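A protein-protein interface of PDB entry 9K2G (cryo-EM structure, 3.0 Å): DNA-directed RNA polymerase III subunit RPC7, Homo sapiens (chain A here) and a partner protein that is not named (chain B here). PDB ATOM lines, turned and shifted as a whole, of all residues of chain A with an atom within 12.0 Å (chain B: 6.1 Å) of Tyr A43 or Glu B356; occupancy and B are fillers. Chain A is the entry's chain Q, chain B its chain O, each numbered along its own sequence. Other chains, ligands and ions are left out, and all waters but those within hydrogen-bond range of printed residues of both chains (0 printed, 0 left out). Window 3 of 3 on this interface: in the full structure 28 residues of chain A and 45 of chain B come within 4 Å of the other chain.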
ATOM      1  N   PHE A  38      13.274 -21.609 -18.855  1.00  0.00           N
ATOM      2  CA  PHE A  38      12.187 -20.689 -19.186  1.00  0.00           C
ATOM      3  C   PHE A  38      12.659 -19.781 -20.316  1.00  0.00           C
ATOM      4  O   PHE A  38      13.259 -18.726 -20.065  1.00  0.00           O
ATOM      5  CB  PHE A  38      11.766 -19.869 -17.965  1.00  0.00           C
ATOM      6  CG  PHE A  38      11.234 -20.696 -16.828  1.00  0.00           C
ATOM      7  CD1 PHE A  38      12.095 -21.237 -15.889  1.00  0.00           C
ATOM      8  CD2 PHE A  38       9.876 -20.924 -16.696  1.00  0.00           C
ATOM      9  CE1 PHE A  38      11.612 -21.996 -14.839  1.00  0.00           C
ATOM     10  CE2 PHE A  38       9.384 -21.681 -15.649  1.00  0.00           C
ATOM     11  CZ  PHE A  38      10.254 -22.221 -14.721  1.00  0.00           C
ATOM     12  N   PRO A  39      12.430 -20.162 -21.572  1.00  0.00           N
ATOM     13  CA  PRO A  39      12.813 -19.284 -22.685  1.00  0.00           C
ATOM     14  C   PRO A  39      12.052 -17.969 -22.626  1.00  0.00           C
ATOM     15  O   PRO A  39      10.869 -17.930 -22.281  1.00  0.00           O
ATOM     16  CB  PRO A  39      12.443 -20.105 -23.927  1.00  0.00           C
ATOM     17  CG  PRO A  39      11.397 -21.063 -23.449  1.00  0.00           C
ATOM     18  CD  PRO A  39      11.771 -21.397 -22.039  1.00  0.00           C
ATOM     19  N   ASP A  40      12.742 -16.886 -22.970  1.00  0.00           N
ATOM     20  CA  ASP A  40      12.145 -15.563 -22.866  1.00  0.00           C
ATOM     21  C   ASP A  40      11.123 -15.333 -23.977  1.00  0.00           C
ATOM     22  O   ASP A  40      11.193 -15.927 -25.053  1.00  0.00           O
ATOM     23  CB  ASP A  40      13.222 -14.477 -22.907  1.00  0.00           C
ATOM     24  CG  ASP A  40      14.090 -14.545 -24.152  1.00  0.00           C
ATOM     25  OD1 ASP A  40      13.937 -15.499 -24.948  1.00  0.00           O
ATOM     26  OD2 ASP A  40      14.935 -13.647 -24.336  1.00  0.00           O
ATOM     27  N   THR A  41      10.155 -14.469 -23.692  1.00  0.00           N
ATOM     28  CA  THR A  41       9.117 -14.093 -24.640  1.00  0.00           C
ATOM     29  C   THR A  41       9.087 -12.576 -24.776  1.00  0.00           C
ATOM     30  O   THR A  41       9.145 -11.857 -23.776  1.00  0.00           O
ATOM     31  CB  THR A  41       7.744 -14.602 -24.195  1.00  0.00           C
ATOM     32  OG1 THR A  41       7.472 -14.139 -22.871  1.00  0.00           O
ATOM     33  CG2 THR A  41       7.709 -16.120 -24.212  1.00  0.00           C
ATOM     34  N   ASP A  42       8.990 -12.097 -26.010  1.00  0.00           N
ATOM     35  CA  ASP A  42       8.930 -10.661 -26.263  1.00  0.00           C
ATOM     36  C   ASP A  42       7.521 -10.097 -26.137  1.00  0.00           C
ATOM     37  O   ASP A  42       7.338  -8.885 -26.290  1.00  0.00           O
ATOM     38  CB  ASP A  42       9.508 -10.327 -27.645  1.00  0.00           C
ATOM     39  CG  ASP A  42       8.713 -10.938 -28.787  1.00  0.00           C
ATOM     40  OD1 ASP A  42       7.820 -11.776 -28.533  1.00  0.00           O
ATOM     41  OD2 ASP A  42       8.993 -10.574 -29.947  1.00  0.00           O
ATOM     42  N   TYR A  43       6.524 -10.943 -25.890  1.00  0.00           N
ATOM     43  CA  TYR A  43       5.171 -10.499 -25.589  1.00  0.00           C
ATOM     44  C   TYR A  43       4.894 -10.694 -24.104  1.00  0.00           C
ATOM     45  O   TYR A  43       5.158 -11.764 -23.549  1.00  0.00           O
ATOM     46  CB  TYR A  43       4.132 -11.274 -26.414  1.00  0.00           C
ATOM     47  CG  TYR A  43       4.232 -11.044 -27.905  1.00  0.00           C
ATOM     48  CD1 TYR A  43       3.795  -9.858 -28.476  1.00  0.00           C
ATOM     49  CD2 TYR A  43       4.751 -12.026 -28.739  1.00  0.00           C
ATOM     50  CE1 TYR A  43       3.882  -9.649 -29.839  1.00  0.00           C
ATOM     51  CE2 TYR A  43       4.838 -11.825 -30.104  1.00  0.00           C
ATOM     52  CZ  TYR A  43       4.405 -10.635 -30.650  1.00  0.00           C
ATOM     53  OH  TYR A  43       4.498 -10.443 -32.009  1.00  0.00           O
ATOM     54  N   LYS A  44       4.366  -9.657 -23.468  1.00  0.00           N
ATOM     55  CA  LYS A  44       4.050  -9.730 -22.051  1.00  0.00           C
ATOM     56  C   LYS A  44       2.539  -9.721 -21.849  1.00  0.00           C
ATOM     57  O   LYS A  44       1.797  -9.229 -22.708  1.00  0.00           O
ATOM     58  CB  LYS A  44       4.682  -8.562 -21.280  1.00  0.00           C
ATOM     59  CG  LYS A  44       6.159  -8.350 -21.588  1.00  0.00           C
ATOM     60  CD  LYS A  44       6.967  -9.640 -21.450  1.00  0.00           C
ATOM     61  CE  LYS A  44       7.082 -10.107 -20.002  1.00  0.00           C
ATOM     62  NZ  LYS A  44       7.909 -11.347 -19.893  1.00  0.00           N
ATOM     63  N   PRO A  45       2.047 -10.271 -20.738  1.00  0.00           N
ATOM     64  CA  PRO A  45       0.599 -10.301 -20.511  1.00  0.00           C
ATOM     65  C   PRO A  45      -0.002  -8.904 -20.484  1.00  0.00           C
ATOM     66  O   PRO A  45       0.610  -7.950 -20.004  1.00  0.00           O
ATOM     67  CB  PRO A  45       0.466 -10.997 -19.151  1.00  0.00           C
ATOM     68  CG  PRO A  45       1.702 -11.823 -19.035  1.00  0.00           C
ATOM     69  CD  PRO A  45       2.782 -11.029 -19.709  1.00  0.00           C
ATOM     70  N   VAL A  46      -1.216  -8.798 -21.021  1.00  0.00           N
ATOM     71  CA  VAL A  46      -1.926  -7.512 -21.045  1.00  0.00           C
ATOM     72  C   VAL A  46      -2.218  -7.079 -19.615  1.00  0.00           C
ATOM     73  O   VAL A  46      -2.585  -7.924 -18.774  1.00  0.00           O
ATOM     74  CB  VAL A  46      -3.222  -7.633 -21.865  1.00  0.00           C
ATOM     75  CG1 VAL A  46      -4.020  -6.333 -21.837  1.00  0.00           C
ATOM     76  CG2 VAL A  46      -2.903  -8.032 -23.299  1.00  0.00           C
ATOM     77  N   PRO A  47      -2.058  -5.801 -19.270  1.00  0.00           N
ATOM     78  CA  PRO A  47      -2.383  -5.359 -17.906  1.00  0.00           C
ATOM     79  C   PRO A  47      -3.847  -5.618 -17.567  1.00  0.00           C
ATOM     80  O   PRO A  47      -4.729  -5.549 -18.424  1.00  0.00           O
ATOM     81  CB  PRO A  47      -2.072  -3.857 -17.931  1.00  0.00           C
ATOM     82  CG  PRO A  47      -1.993  -3.490 -19.383  1.00  0.00           C
ATOM     83  CD  PRO A  47      -1.477  -4.713 -20.071  1.00  0.00           C
ATOM     84  N   LEU A  48      -4.083  -5.926 -16.296  1.00  0.00           N
ATOM     85  CA  LEU A  48      -5.405  -6.322 -15.837  1.00  0.00           C
ATOM     86  C   LEU A  48      -6.396  -5.167 -15.945  1.00  0.00           C
ATOM     87  O   LEU A  48      -6.032  -3.991 -15.854  1.00  0.00           O
ATOM     88  CB  LEU A  48      -5.345  -6.820 -14.393  1.00  0.00           C
ATOM     89  CG  LEU A  48      -4.943  -8.277 -14.148  1.00  0.00           C
ATOM     90  CD1 LEU A  48      -5.888  -9.218 -14.875  1.00  0.00           C
ATOM     91  CD2 LEU A  48      -3.500  -8.535 -14.562  1.00  0.00           C
ATOM     92  N   LYS A  49      -7.662  -5.520 -16.144  1.00  0.00           N
ATOM     93  CA  LYS A  49      -8.725  -4.527 -16.187  1.00  0.00           C
ATOM     94  C   LYS A  49      -8.877  -3.860 -14.826  1.00  0.00           C
ATOM     95  O   LYS A  49      -8.734  -4.501 -13.782  1.00  0.00           O
ATOM     96  CB  LYS A  49     -10.040  -5.170 -16.613  1.00  0.00           C
ATOM     97  CG  LYS A  49      -9.952  -5.964 -17.909  1.00  0.00           C
ATOM     98  CD  LYS A  49     -11.302  -6.551 -18.283  1.00  0.00           C
ATOM     99  CE  LYS A  49     -12.352  -5.464 -18.420  1.00  0.00           C
ATOM    100  NZ  LYS A  49     -11.927  -4.403 -19.375  1.00  0.00           N
ATOM    101  N   GLU B 351      -9.357 -15.026 -31.961  1.00  0.00           N
ATOM    102  CA  GLU B 351      -8.474 -14.115 -32.680  1.00  0.00           C
ATOM    103  C   GLU B 351      -7.717 -13.209 -31.718  1.00  0.00           C
ATOM    104  O   GLU B 351      -6.548 -12.897 -31.963  1.00  0.00           O
ATOM    105  CB  GLU B 351      -9.262 -13.299 -33.707  1.00  0.00           C
ATOM    106  CG  GLU B 351     -10.007 -12.094 -33.155  1.00  0.00           C
ATOM    107  CD  GLU B 351     -10.663 -11.263 -34.239  1.00  0.00           C
ATOM    108  OE1 GLU B 351     -10.906 -11.805 -35.340  1.00  0.00           O
ATOM    109  OE2 GLU B 351     -10.929 -10.068 -33.995  1.00  0.00           O
ATOM    110  N   SER B 352      -8.346 -12.804 -30.611  1.00  0.00           N
ATOM    111  CA  SER B 352      -7.665 -11.965 -29.634  1.00  0.00           C
ATOM    112  C   SER B 352      -6.526 -12.712 -28.955  1.00  0.00           C
ATOM    113  O   SER B 352      -5.433 -12.157 -28.780  1.00  0.00           O
ATOM    114  CB  SER B 352      -8.661 -11.455 -28.597  1.00  0.00           C
ATOM    115  OG  SER B 352      -8.006 -10.699 -27.592  1.00  0.00           O
ATOM    116  N   VAL B 353      -6.755 -13.969 -28.564  1.00  0.00           N
ATOM    117  CA  VAL B 353      -5.686 -14.718 -27.909  1.00  0.00           C
ATOM    118  C   VAL B 353      -4.560 -15.015 -28.893  1.00  0.00           C
ATOM    119  O   VAL B 353      -3.376 -14.947 -28.537  1.00  0.00           O
ATOM    120  CB  VAL B 353      -6.229 -15.999 -27.238  1.00  0.00           C
ATOM    121  CG1 VAL B 353      -6.862 -16.939 -28.244  1.00  0.00           C
ATOM    122  CG2 VAL B 353      -5.118 -16.714 -26.473  1.00  0.00           C
ATOM    123  N   VAL B 354      -4.898 -15.308 -30.154  1.00  0.00           N
ATOM    124  CA  VAL B 354      -3.862 -15.509 -31.166  1.00  0.00           C
ATOM    125  C   VAL B 354      -3.047 -14.234 -31.359  1.00  0.00           C
ATOM    126  O   VAL B 354      -1.811 -14.273 -31.423  1.00  0.00           O
ATOM    127  CB  VAL B 354      -4.489 -15.994 -32.488  1.00  0.00           C
ATOM    128  CG1 VAL B 354      -3.496 -15.843 -33.631  1.00  0.00           C
ATOM    129  CG2 VAL B 354      -4.934 -17.445 -32.363  1.00  0.00           C
ATOM    130  N   GLN B 355      -3.724 -13.086 -31.443  1.00  0.00           N
ATOM    131  CA  GLN B 355      -3.028 -11.821 -31.635  1.00  0.00           C
ATOM    132  C   GLN B 355      -2.108 -11.505 -30.460  1.00  0.00           C
ATOM    133  O   GLN B 355      -0.959 -11.083 -30.657  1.00  0.00           O
ATOM    134  CB  GLN B 355      -4.033 -10.690 -31.841  1.00  0.00           C
ATOM    135  CG  GLN B 355      -3.411  -9.304 -31.839  1.00  0.00           C
ATOM    136  CD  GLN B 355      -4.267  -8.284 -32.563  1.00  0.00           C
ATOM    137  OE1 GLN B 355      -5.253  -8.630 -33.210  1.00  0.00           O
ATOM    138  NE2 GLN B 355      -3.891  -7.015 -32.461  1.00  0.00           N
ATOM    139  N   GLU B 356      -2.586 -11.701 -29.234  1.00  0.00           N
ATOM    140  CA  GLU B 356      -1.771 -11.379 -28.071  1.00  0.00           C
ATOM    141  C   GLU B 356      -0.661 -12.389 -27.822  1.00  0.00           C
ATOM    142  O   GLU B 356       0.321 -12.052 -27.150  1.00  0.00           O
ATOM    143  CB  GLU B 356      -2.646 -11.247 -26.825  1.00  0.00           C
ATOM    144  CG  GLU B 356      -3.309  -9.892 -26.689  1.00  0.00           C
ATOM    145  CD  GLU B 356      -2.303  -8.754 -26.696  1.00  0.00           C
ATOM    146  OE1 GLU B 356      -1.239  -8.899 -26.059  1.00  0.00           O
ATOM    147  OE2 GLU B 356      -2.574  -7.726 -27.344  1.00  0.00           O
ATOM    148  N   ARG B 357      -0.781 -13.610 -28.342  1.00  0.00           N
ATOM    149  CA  ARG B 357       0.263 -14.599 -28.121  1.00  0.00           C
ATOM    150  C   ARG B 357       1.298 -14.641 -29.238  1.00  0.00           C
ATOM    151  O   ARG B 357       2.441 -15.046 -28.996  1.00  0.00           O
ATOM    152  CB  ARG B 357      -0.357 -15.988 -27.942  1.00  0.00           C
ATOM    153  CG  ARG B 357       0.589 -17.020 -27.354  1.00  0.00           C
ATOM    154  CD  ARG B 357      -0.055 -18.386 -27.289  1.00  0.00           C
ATOM    155  NE  ARG B 357       0.936 -19.436 -27.071  1.00  0.00           N
ATOM    156  CZ  ARG B 357       0.680 -20.733 -27.156  1.00  0.00           C
ATOM    157  NH1 ARG B 357      -0.531 -21.183 -27.446  1.00  0.00           N
ATOM    158  NH2 ARG B 357       1.663 -21.603 -26.948  1.00  0.00           N
ATOM    159  N   PHE B 358       0.944 -14.223 -30.459  1.00  0.00           N
ATOM    160  CA  PHE B 358       1.872 -14.309 -31.572  1.00  0.00           C
ATOM    161  C   PHE B 358       1.981 -13.038 -32.412  1.00  0.00           C
ATOM    162  O   PHE B 358       2.705 -13.044 -33.412  1.00  0.00           O
ATOM    163  CB  PHE B 358       1.500 -15.481 -32.494  1.00  0.00           C
ATOM    164  CG  PHE B 358       1.449 -16.806 -31.799  1.00  0.00           C
ATOM    165  CD1 PHE B 358       2.586 -17.359 -31.239  1.00  0.00           C
ATOM    166  CD2 PHE B 358       0.257 -17.514 -31.717  1.00  0.00           C
ATOM    167  CE1 PHE B 358       2.542 -18.582 -30.599  1.00  0.00           C
ATOM    168  CE2 PHE B 358       0.207 -18.742 -31.083  1.00  0.00           C
ATOM    169  CZ  PHE B 358       1.350 -19.274 -30.526  1.00  0.00           C
ATOM    170  N   GLY B 359       1.295 -11.962 -32.045  1.00  0.00           N
ATOM    171  CA  GLY B 359       1.414 -10.698 -32.742  1.00  0.00           C
ATOM    172  C   GLY B 359       0.310 -10.473 -33.761  1.00  0.00           C
ATOM    173  O   GLY B 359      -0.500 -11.350 -34.067  1.00  0.00           O
ATOM    174  N   SER B 360       0.293  -9.245 -34.289  1.00  0.00           N
ATOM    175  CA  SER B 360      -0.779  -8.834 -35.190  1.00  0.00           C
ATOM    176  C   SER B 360      -0.658  -9.508 -36.559  1.00  0.00           C
ATOM    177  O   SER B 360      -1.678  -9.777 -37.209  1.00  0.00           O
ATOM    178  CB  SER B 360      -0.779  -7.308 -35.341  1.00  0.00           C
ATOM    179  OG  SER B 360      -1.103  -6.680 -34.103  1.00  0.00           O
ATOM    180  N   MET B 394       5.020 -18.881 -38.927  1.00  0.00           N
ATOM    181  CA  MET B 394       3.885 -18.624 -38.047  1.00  0.00           C
ATOM    182  C   MET B 394       2.791 -19.672 -38.233  1.00  0.00           C
ATOM    183  O   MET B 394       2.138 -20.069 -37.260  1.00  0.00           O
ATOM    184  CB  MET B 394       3.344 -17.216 -38.281  1.00  0.00           C
ATOM    185  CG  MET B 394       4.271 -16.119 -37.773  1.00  0.00           C
ATOM    186  SD  MET B 394       3.513 -14.487 -37.763  1.00  0.00           S
ATOM    187  CE  MET B 394       4.657 -13.603 -36.702  1.00  0.00           C
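Of the 11 printed residues of chain B, 4 touch a printed residue of chain A.
Of the 12 printed residues of chain A, 2 touch a printed residue of chain B.
Of chain B, only Glu B356 (3.96 Å), Arg B357 (3.8 Å), Phe B358 (3.5 Å) and Gly B359 (3.2 Å) come within 4 Å of Tyr A43.
Glu B356 touches just these residues of chain A: Tyr A43 (3.96 Å) and Val A46 (3.3 Å).
No residue of chain A comes within 4 Å of Ser B352.
Gln B355 touches none of the printed residues of chain A.
Of chain A, only Tyr A43 (3.5 Å) comes within 4 Å of Phe B358.
Printed residues of chain B within 4 Å of Val A46: Glu B356 (3.3 Å).
Of the printed residues of chain A, Arg B357 touches Tyr A43.
The side-chain hydroxyl (OG1) of Thr A41 sits at hydrogen-bond distance from the backbone carbonyl oxygen (O) of Tyr A43, at 3.4 Å.
The backbone carbonyl oxygen (O) of Phe B358 is in hydrogen-bond range of the side-chain hydroxyl (OH) of Tyr A43.
Among the printed residues, pairs that only touch across the chains: Tyr A43 with Gly B359, Val A46 with Glu B356, Tyr A43 with Arg B357 and Tyr A43 with Glu B356.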
